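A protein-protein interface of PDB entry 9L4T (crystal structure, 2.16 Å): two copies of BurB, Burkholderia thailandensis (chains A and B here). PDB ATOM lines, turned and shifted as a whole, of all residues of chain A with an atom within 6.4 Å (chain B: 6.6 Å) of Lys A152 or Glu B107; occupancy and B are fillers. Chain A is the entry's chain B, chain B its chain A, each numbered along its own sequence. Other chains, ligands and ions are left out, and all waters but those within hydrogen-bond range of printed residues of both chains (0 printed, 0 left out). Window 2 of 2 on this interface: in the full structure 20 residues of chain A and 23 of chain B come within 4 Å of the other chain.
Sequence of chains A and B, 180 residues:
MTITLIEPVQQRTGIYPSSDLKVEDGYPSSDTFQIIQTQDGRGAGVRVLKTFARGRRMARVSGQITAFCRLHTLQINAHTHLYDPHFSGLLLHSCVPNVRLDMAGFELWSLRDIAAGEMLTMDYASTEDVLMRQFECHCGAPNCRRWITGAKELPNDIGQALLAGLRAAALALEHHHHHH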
ATOM      1  N   ALA A  78      34.959   8.406  -8.012  1.00  0.00           N
ATOM      2  CA  ALA A  78      35.247   7.225  -7.199  1.00  0.00           C
ATOM      3  C   ALA A  78      36.129   7.543  -5.990  1.00  0.00           C
ATOM      4  O   ALA A  78      36.048   6.847  -4.968  1.00  0.00           O
ATOM      5  CB  ALA A  78      35.892   6.140  -8.065  1.00  0.00           C
ATOM      6  N   ALA A 125      21.860   7.553  -1.184  1.00  0.00           N
ATOM      7  CA  ALA A 125      22.424   6.451  -1.937  1.00  0.00           C
ATOM      8  C   ALA A 125      22.499   6.741  -3.427  1.00  0.00           C
ATOM      9  O   ALA A 125      23.181   6.002  -4.147  1.00  0.00           O
ATOM     10  CB  ALA A 125      21.612   5.181  -1.688  1.00  0.00           C
ATOM     11  N   GLU A 128      26.175   8.594  -2.998  1.00  0.00           N
ATOM     12  CA  GLU A 128      27.207   8.169  -2.047  1.00  0.00           C
ATOM     13  C   GLU A 128      27.442   6.658  -2.116  1.00  0.00           C
ATOM     14  O   GLU A 128      26.499   5.872  -1.938  1.00  0.00           O
ATOM     15  CB  GLU A 128      26.814   8.580  -0.628  1.00  0.00           C
ATOM     16  CG  GLU A 128      26.509  10.069  -0.464  1.00  0.00           C
ATOM     17  CD  GLU A 128      27.649  10.969  -0.990  1.00  0.00           C
ATOM     18  OE1 GLU A 128      28.765  10.889  -0.439  1.00  0.00           O
ATOM     19  OE2 GLU A 128      27.431  11.735  -1.957  1.00  0.00           O
ATOM     20  N   ASP A 129      28.702   6.259  -2.375  1.00  0.00           N
ATOM     21  CA  ASP A 129      29.094   4.842  -2.325  1.00  0.00           C
ATOM     22  C   ASP A 129      28.878   4.258  -0.936  1.00  0.00           C
ATOM     23  O   ASP A 129      28.344   3.149  -0.778  1.00  0.00           O
ATOM     24  CB  ASP A 129      30.583   4.682  -2.675  1.00  0.00           C
ATOM     25  CG  ASP A 129      30.874   4.774  -4.165  1.00  0.00           C
ATOM     26  OD1 ASP A 129      29.927   4.891  -4.984  1.00  0.00           O
ATOM     27  OD2 ASP A 129      32.081   4.723  -4.501  1.00  0.00           O
ATOM     28  N   VAL A 130      29.397   4.960   0.078  1.00  0.00           N
ATOM     29  CA  VAL A 130      29.331   4.591   1.484  1.00  0.00           C
ATOM     30  C   VAL A 130      29.114   5.881   2.263  1.00  0.00           C
ATOM     31  O   VAL A 130      29.378   6.981   1.769  1.00  0.00           O
ATOM     32  CB  VAL A 130      30.609   3.870   1.985  1.00  0.00           C
ATOM     33  CG1 VAL A 130      31.081   2.820   0.993  1.00  0.00           C
ATOM     34  CG2 VAL A 130      31.708   4.881   2.247  1.00  0.00           C
ATOM     35  N   THR A 149      22.237   3.238   4.048  1.00  0.00           N
ATOM     36  CA  THR A 149      23.643   3.031   3.755  1.00  0.00           C
ATOM     37  C   THR A 149      23.940   3.714   2.429  1.00  0.00           C
ATOM     38  O   THR A 149      23.031   4.161   1.717  1.00  0.00           O
ATOM     39  CB  THR A 149      24.009   1.532   3.673  1.00  0.00           C
ATOM     40  OG1 THR A 149      23.473   0.961   2.472  1.00  0.00           O
ATOM     41  CG2 THR A 149      23.481   0.754   4.866  1.00  0.00           C
ATOM     42  N   GLY A 150      25.227   3.794   2.099  1.00  0.00           N
ATOM     43  CA  GLY A 150      25.619   4.112   0.737  1.00  0.00           C
ATOM     44  C   GLY A 150      25.093   3.062  -0.223  1.00  0.00           C
ATOM     45  O   GLY A 150      24.619   1.992   0.162  1.00  0.00           O
ATOM     46  N   ALA A 151      25.186   3.377  -1.517  1.00  0.00           N
ATOM     47  CA  ALA A 151      24.726   2.428  -2.520  1.00  0.00           C
ATOM     48  C   ALA A 151      25.617   1.192  -2.578  1.00  0.00           C
ATOM     49  O   ALA A 151      25.137   0.112  -2.924  1.00  0.00           O
ATOM     50  CB  ALA A 151      24.637   3.105  -3.895  1.00  0.00           C
ATOM     51  N   LYS A 152      26.903   1.306  -2.237  1.00  0.00           N
ATOM     52  CA  LYS A 152      27.806   0.161  -2.340  1.00  0.00           C
ATOM     53  C   LYS A 152      28.161  -0.431  -0.978  1.00  0.00           C
ATOM     54  O   LYS A 152      29.158  -1.149  -0.853  1.00  0.00           O
ATOM     55  CB  LYS A 152      29.071   0.548  -3.125  1.00  0.00           C
ATOM     56  CG  LYS A 152      28.758   1.092  -4.525  1.00  0.00           C
ATOM     57  CD  LYS A 152      30.025   1.313  -5.359  1.00  0.00           C
ATOM     58  CE  LYS A 152      29.716   1.912  -6.718  1.00  0.00           C
ATOM     59  NZ  LYS A 152      30.974   2.145  -7.514  1.00  0.00           N
ATOM     60  N   GLU A 153      27.333  -0.192   0.036  1.00  0.00           N
ATOM     61  CA  GLU A 153      27.672  -0.469   1.424  1.00  0.00           C
ATOM     62  C   GLU A 153      26.686  -1.454   2.034  1.00  0.00           C
ATOM     63  O   GLU A 153      25.471  -1.242   1.968  1.00  0.00           O
ATOM     64  CB  GLU A 153      27.654   0.824   2.222  1.00  0.00           C
ATOM     65  CG  GLU A 153      28.108   0.695   3.628  1.00  0.00           C
ATOM     66  CD  GLU A 153      28.075   2.032   4.301  1.00  0.00           C
ATOM     67  OE1 GLU A 153      27.419   2.939   3.739  1.00  0.00           O
ATOM     68  OE2 GLU A 153      28.681   2.172   5.385  1.00  0.00           O
ATOM     69  N   LEU A 154      27.207  -2.508   2.650  1.00  0.00           N
ATOM     70  CA  LEU A 154      26.326  -3.450   3.327  1.00  0.00           C
ATOM     71  C   LEU A 154      25.886  -2.888   4.677  1.00  0.00           C
ATOM     72  O   LEU A 154      26.649  -2.167   5.326  1.00  0.00           O
ATOM     73  CB  LEU A 154      27.030  -4.787   3.533  1.00  0.00           C
ATOM     74  CG  LEU A 154      27.286  -5.612   2.271  1.00  0.00           C
ATOM     75  CD1 LEU A 154      27.835  -6.962   2.660  1.00  0.00           C
ATOM     76  CD2 LEU A 154      26.005  -5.768   1.469  1.00  0.00           C
ATOM     77  N   GLY B  55      22.807  -3.973  -1.515  1.00  0.00           N
ATOM     78  CA  GLY B  55      24.186  -3.527  -1.357  1.00  0.00           C
ATOM     79  C   GLY B  55      25.196  -4.453  -1.993  1.00  0.00           C
ATOM     80  O   GLY B  55      26.298  -4.636  -1.455  1.00  0.00           O
ATOM     81  N   ARG B  56      24.844  -5.054  -3.128  1.00  0.00           N
ATOM     82  CA  ARG B  56      25.725  -5.956  -3.849  1.00  0.00           C
ATOM     83  C   ARG B  56      25.803  -5.520  -5.298  1.00  0.00           C
ATOM     84  O   ARG B  56      24.828  -5.006  -5.860  1.00  0.00           O
ATOM     85  CB  ARG B  56      25.233  -7.414  -3.780  1.00  0.00           C
ATOM     86  CG  ARG B  56      25.912  -8.262  -2.707  1.00  0.00           C
ATOM     87  CD  ARG B  56      25.456  -9.714  -2.806  1.00  0.00           C
ATOM     88  NE  ARG B  56      25.995 -10.369  -3.998  1.00  0.00           N
ATOM     89  CZ  ARG B  56      25.379 -11.339  -4.667  1.00  0.00           C
ATOM     90  NH1 ARG B  56      24.207 -11.823  -4.272  1.00  0.00           N
ATOM     91  NH2 ARG B  56      25.951 -11.838  -5.760  1.00  0.00           N
ATOM     92  N   ARG B  57      26.971  -5.734  -5.900  1.00  0.00           N
ATOM     93  CA  ARG B  57      27.108  -5.542  -7.337  1.00  0.00           C
ATOM     94  C   ARG B  57      26.446  -6.710  -8.056  1.00  0.00           C
ATOM     95  O   ARG B  57      26.839  -7.866  -7.874  1.00  0.00           O
ATOM     96  CB  ARG B  57      28.580  -5.409  -7.733  1.00  0.00           C
ATOM     97  CG  ARG B  57      28.824  -4.977  -9.181  1.00  0.00           C
ATOM     98  CD  ARG B  57      30.301  -5.092  -9.514  1.00  0.00           C
ATOM     99  NE  ARG B  57      30.675  -6.424  -9.984  1.00  0.00           N
ATOM    100  CZ  ARG B  57      31.923  -6.872 -10.070  1.00  0.00           C
ATOM    101  NH1 ARG B  57      32.954  -6.125  -9.712  1.00  0.00           N
ATOM    102  NH2 ARG B  57      32.143  -8.108 -10.513  1.00  0.00           N
ATOM    103  N   MET B  58      25.410  -6.408  -8.841  1.00  0.00           N
ATOM    104  CA  MET B  58      24.697  -7.418  -9.611  1.00  0.00           C
ATOM    105  C   MET B  58      25.298  -7.661 -10.983  1.00  0.00           C
ATOM    106  O   MET B  58      25.121  -8.758 -11.524  1.00  0.00           O
ATOM    107  CB  MET B  58      23.227  -7.019  -9.797  1.00  0.00           C
ATOM    108  CG  MET B  58      22.662  -6.229  -8.630  1.00  0.00           C
ATOM    109  SD  MET B  58      20.891  -5.892  -8.748  1.00  0.00           S
ATOM    110  CE  MET B  58      20.203  -7.471  -9.234  1.00  0.00           C
ATOM    111  N   ALA B  59      25.975  -6.670 -11.570  1.00  0.00           N
ATOM    112  CA  ALA B  59      26.519  -6.830 -12.914  1.00  0.00           C
ATOM    113  C   ALA B  59      27.450  -5.671 -13.250  1.00  0.00           C
ATOM    114  O   ALA B  59      27.244  -4.541 -12.786  1.00  0.00           O
ATOM    115  CB  ALA B  59      25.399  -6.896 -13.953  1.00  0.00           C
ATOM    116  N   ARG B  60      28.469  -5.958 -14.066  1.00  0.00           N
ATOM    117  CA  ARG B  60      29.151  -4.884 -14.771  1.00  0.00           C
ATOM    118  C   ARG B  60      28.357  -4.531 -16.019  1.00  0.00           C
ATOM    119  O   ARG B  60      27.732  -5.390 -16.645  1.00  0.00           O
ATOM    120  CB  ARG B  60      30.583  -5.265 -15.157  1.00  0.00           C
ATOM    121  CG  ARG B  60      31.574  -5.406 -14.001  1.00  0.00           C
ATOM    122  CD  ARG B  60      33.014  -5.589 -14.557  1.00  0.00           C
ATOM    123  NE  ARG B  60      33.984  -6.088 -13.580  1.00  0.00           N
ATOM    124  CZ  ARG B  60      34.669  -5.304 -12.761  1.00  0.00           C
ATOM    125  NH1 ARG B  60      34.486  -3.994 -12.752  1.00  0.00           N
ATOM    126  NH2 ARG B  60      35.545  -5.847 -11.921  1.00  0.00           N
ATOM    127  N   VAL B  61      28.385  -3.255 -16.378  1.00  0.00           N
ATOM    128  CA  VAL B  61      27.639  -2.738 -17.514  1.00  0.00           C
ATOM    129  C   VAL B  61      28.603  -2.378 -18.637  1.00  0.00           C
ATOM    130  O   VAL B  61      29.764  -2.017 -18.396  1.00  0.00           O
ATOM    131  CB  VAL B  61      26.797  -1.522 -17.067  1.00  0.00           C
ATOM    132  CG1 VAL B  61      26.222  -0.775 -18.266  1.00  0.00           C
ATOM    133  CG2 VAL B  61      25.691  -1.998 -16.117  1.00  0.00           C
ATOM    134  N   ARG B 100      20.340   0.470  -8.675  1.00  0.00           N
ATOM    135  CA  ARG B 100      20.969   1.732  -9.024  1.00  0.00           C
ATOM    136  C   ARG B 100      22.045   1.508 -10.081  1.00  0.00           C
ATOM    137  O   ARG B 100      22.862   0.584  -9.978  1.00  0.00           O
ATOM    138  CB  ARG B 100      21.595   2.404  -7.807  1.00  0.00           C
ATOM    139  CG  ARG B 100      21.972   3.831  -8.103  1.00  0.00           C
ATOM    140  CD  ARG B 100      23.028   4.409  -7.197  1.00  0.00           C
ATOM    141  NE  ARG B 100      23.742   5.426  -7.963  1.00  0.00           N
ATOM    142  CZ  ARG B 100      24.851   6.043  -7.587  1.00  0.00           C
ATOM    143  NH1 ARG B 100      25.334   5.910  -6.355  1.00  0.00           N
ATOM    144  NH2 ARG B 100      25.482   6.829  -8.465  1.00  0.00           N
ATOM    145  N   LEU B 101      22.037   2.357 -11.095  1.00  0.00           N
ATOM    146  CA  LEU B 101      23.079   2.347 -12.115  1.00  0.00           C
ATOM    147  C   LEU B 101      24.170   3.340 -11.710  1.00  0.00           C
ATOM    148  O   LEU B 101      23.901   4.531 -11.511  1.00  0.00           O
ATOM    149  CB  LEU B 101      22.486   2.706 -13.476  1.00  0.00           C
ATOM    150  CG  LEU B 101      22.871   1.963 -14.745  1.00  0.00           C
ATOM    151  CD1 LEU B 101      23.058   0.480 -14.519  1.00  0.00           C
ATOM    152  CD2 LEU B 101      21.769   2.199 -15.737  1.00  0.00           C
ATOM    153  N   ASP B 102      25.382   2.845 -11.554  1.00  0.00           N
ATOM    154  CA  ASP B 102      26.535   3.679 -11.276  1.00  0.00           C
ATOM    155  C   ASP B 102      27.222   3.959 -12.614  1.00  0.00           C
ATOM    156  O   ASP B 102      27.812   3.055 -13.215  1.00  0.00           O
ATOM    157  CB  ASP B 102      27.436   2.961 -10.275  1.00  0.00           C
ATOM    158  CG  ASP B 102      28.884   3.414 -10.333  1.00  0.00           C
ATOM    159  OD1 ASP B 102      29.163   4.604 -10.656  1.00  0.00           O
ATOM    160  OD2 ASP B 102      29.744   2.541 -10.035  1.00  0.00           O
ATOM    161  N   MET B 103      27.126   5.197 -13.098  1.00  0.00           N
ATOM    162  CA  MET B 103      27.661   5.536 -14.409  1.00  0.00           C
ATOM    163  C   MET B 103      29.103   6.048 -14.358  1.00  0.00           C
ATOM    164  O   MET B 103      29.613   6.506 -15.384  1.00  0.00           O
ATOM    165  CB  MET B 103      26.761   6.561 -15.112  1.00  0.00           C
ATOM    166  CG  MET B 103      25.324   6.093 -15.376  1.00  0.00           C
ATOM    167  SD  MET B 103      25.255   4.612 -16.421  1.00  0.00           S
ATOM    168  CE  MET B 103      25.938   5.272 -17.945  1.00  0.00           C
ATOM    169  N   ALA B 104      29.762   5.997 -13.200  1.00  0.00           N
ATOM    170  CA  ALA B 104      31.198   6.262 -13.121  1.00  0.00           C
ATOM    171  C   ALA B 104      31.983   4.963 -13.163  1.00  0.00           C
ATOM    172  O   ALA B 104      32.952   4.829 -13.927  1.00  0.00           O
ATOM    173  CB  ALA B 104      31.532   7.034 -11.839  1.00  0.00           C
ATOM    174  N   GLY B 105      31.553   3.988 -12.371  1.00  0.00           N
ATOM    175  CA  GLY B 105      32.130   2.662 -12.421  1.00  0.00           C
ATOM    176  C   GLY B 105      31.488   1.699 -13.388  1.00  0.00           C
ATOM    177  O   GLY B 105      32.013   0.593 -13.569  1.00  0.00           O
ATOM    178  N   PHE B 106      30.361   2.076 -14.002  1.00  0.00           N
ATOM    179  CA  PHE B 106      29.625   1.222 -14.949  1.00  0.00           C
ATOM    180  C   PHE B 106      29.263  -0.140 -14.329  1.00  0.00           C
ATOM    181  O   PHE B 106      29.776  -1.201 -14.720  1.00  0.00           O
ATOM    182  CB  PHE B 106      30.427   1.076 -16.252  1.00  0.00           C
ATOM    183  CG  PHE B 106      30.480   2.355 -17.056  1.00  0.00           C
ATOM    184  CD1 PHE B 106      31.339   3.376 -16.694  1.00  0.00           C
ATOM    185  CD2 PHE B 106      29.611   2.555 -18.119  1.00  0.00           C
ATOM    186  CE1 PHE B 106      31.365   4.570 -17.405  1.00  0.00           C
ATOM    187  CE2 PHE B 106      29.627   3.726 -18.835  1.00  0.00           C
ATOM    188  CZ  PHE B 106      30.503   4.740 -18.477  1.00  0.00           C
ATOM    189  N   GLU B 107      28.324  -0.094 -13.372  1.00  0.00           N
ATOM    190  CA  GLU B 107      27.919  -1.261 -12.581  1.00  0.00           C
ATOM    191  C   GLU B 107      26.474  -1.114 -12.117  1.00  0.00           C
ATOM    192  O   GLU B 107      25.995  -0.005 -11.855  1.00  0.00           O
ATOM    193  CB  GLU B 107      28.808  -1.475 -11.339  1.00  0.00           C
ATOM    194  CG  GLU B 107      30.311  -1.694 -11.649  1.00  0.00           C
ATOM    195  CD  GLU B 107      31.198  -1.773 -10.421  1.00  0.00           C
ATOM    196  OE1 GLU B 107      30.749  -1.362  -9.319  1.00  0.00           O
ATOM    197  OE2 GLU B 107      32.351  -2.255 -10.567  1.00  0.00           O
ATOM    198  N   LEU B 108      25.796  -2.259 -11.981  1.00  0.00           N
ATOM    199  CA  LEU B 108      24.425  -2.333 -11.478  1.00  0.00           C
ATOM    200  C   LEU B 108      24.454  -2.817 -10.029  1.00  0.00           C
ATOM    201  O   LEU B 108      24.955  -3.914  -9.757  1.00  0.00           O
ATOM    202  CB  LEU B 108      23.594  -3.279 -12.345  1.00  0.00           C
ATOM    203  CG  LEU B 108      22.067  -3.198 -12.164  1.00  0.00           C
ATOM    204  CD1 LEU B 108      21.583  -1.744 -12.214  1.00  0.00           C
ATOM    205  CD2 LEU B 108      21.341  -4.037 -13.200  1.00  0.00           C
ATOM    206  N   TRP B 109      23.937  -2.002  -9.099  1.00  0.00           N
ATOM    207  CA  TRP B 109      23.908  -2.356  -7.676  1.00  0.00           C
ATOM    208  C   TRP B 109      22.473  -2.459  -7.150  1.00  0.00           C
ATOM    209  O   TRP B 109      21.581  -1.706  -7.562  1.00  0.00           O
ATOM    210  CB  TRP B 109      24.684  -1.341  -6.821  1.00  0.00           C
ATOM    211  CG  TRP B 109      26.188  -1.452  -6.946  1.00  0.00           C
ATOM    212  CD1 TRP B 109      26.953  -1.031  -8.001  1.00  0.00           C
ATOM    213  CD2 TRP B 109      27.100  -1.989  -5.974  1.00  0.00           C
ATOM    214  NE1 TRP B 109      28.288  -1.290  -7.755  1.00  0.00           N
ATOM    215  CE2 TRP B 109      28.406  -1.875  -6.517  1.00  0.00           C
ATOM    216  CE3 TRP B 109      26.943  -2.557  -4.700  1.00  0.00           C
ATOM    217  CZ2 TRP B 109      29.544  -2.316  -5.833  1.00  0.00           C
ATOM    218  CZ3 TRP B 109      28.074  -2.998  -4.024  1.00  0.00           C
ATOM    219  CH2 TRP B 109      29.356  -2.879  -4.592  1.00  0.00           C
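The guanidinium group of Arg B100 lies within hydrogen-bond range of the backbone carbonyl oxygen of Ala A125, 3.1 Å away.
The side-chain carboxylate (OD2) of Asp B102 lies within salt-bridge range of the side-chain amino group (NZ) of Lys A152 (2.8 Å).
OE1 of Glu B107 is in salt-bridge range of NZ of Lys A152 (3.95 Å).
The backbone NH of Arg B100 is in hydrogen-bond range of the backbone carbonyl oxygen of Trp B109, 2.7 Å away.
The backbone NH of Gly B105 sits at hydrogen-bond distance from the side-chain carboxylate of Asp B102 (3.0 Å).
OE1 of Glu B107 lies within hydrogen-bond range of NE1 of Trp B109, 2.9 Å away.
The backbone carbonyl oxygen of Glu A128 lies within hydrogen-bond range of the backbone NH of Ala A151.
The backbone carbonyl oxygen (O) of Asp A129 sits at hydrogen-bond distance from the backbone NH (N) of Ala A151, at 3.3 Å.
The side-chain carboxylate (OD1) of Asp A129 is in salt-bridge range of the side-chain amino group (NZ) of Lys A152.
Ala A151 touches Arg B100.
Ala A151 touches Trp B109.
Lys A152 touches Trp B109 (CA to CZ3, 3.6 Å).
Gly B55 touches Leu A154 (O to CD2, 3.1 Å).
Of chain B, only Asp B102, Glu B107 and Trp B109 come within 4 Å of Lys A152.
Of the printed residues of chain B, Ala A125 touches Arg B100.
Printed residues of chain A within 4 Å of Asp B102: Lys A152 (2.8 Å).
Of the printed residues of chain B, Leu A154 touches Gly B55 (3.1 Å).
Arg B60 touches none of the printed residues of chain A.
The nearest printed residue of chain A that does not touch Trp B109 is Glu A153 (5.0 Å).
Of the 17 printed residues of chain B, 5 touch a printed residue of chain A.
Of the 11 printed residues of chain A, 4 touch a printed residue of chain B.
Printed residues of chain A that touch a printed residue of chain B: Ala A125, Ala A151, Lys A152 and Leu A154.
Among the printed residues, Asp or Glu carboxylates within 4 Å of a Lys or Arg side-chain nitrogen of the other chain: Lys A152 with Asp B102 and Lys A152 with Glu B107.
No position is printed for both chains.
Of the 7 pairs that touch across the chains among the printed residues, none has its exchanged pair printed and touching as well.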
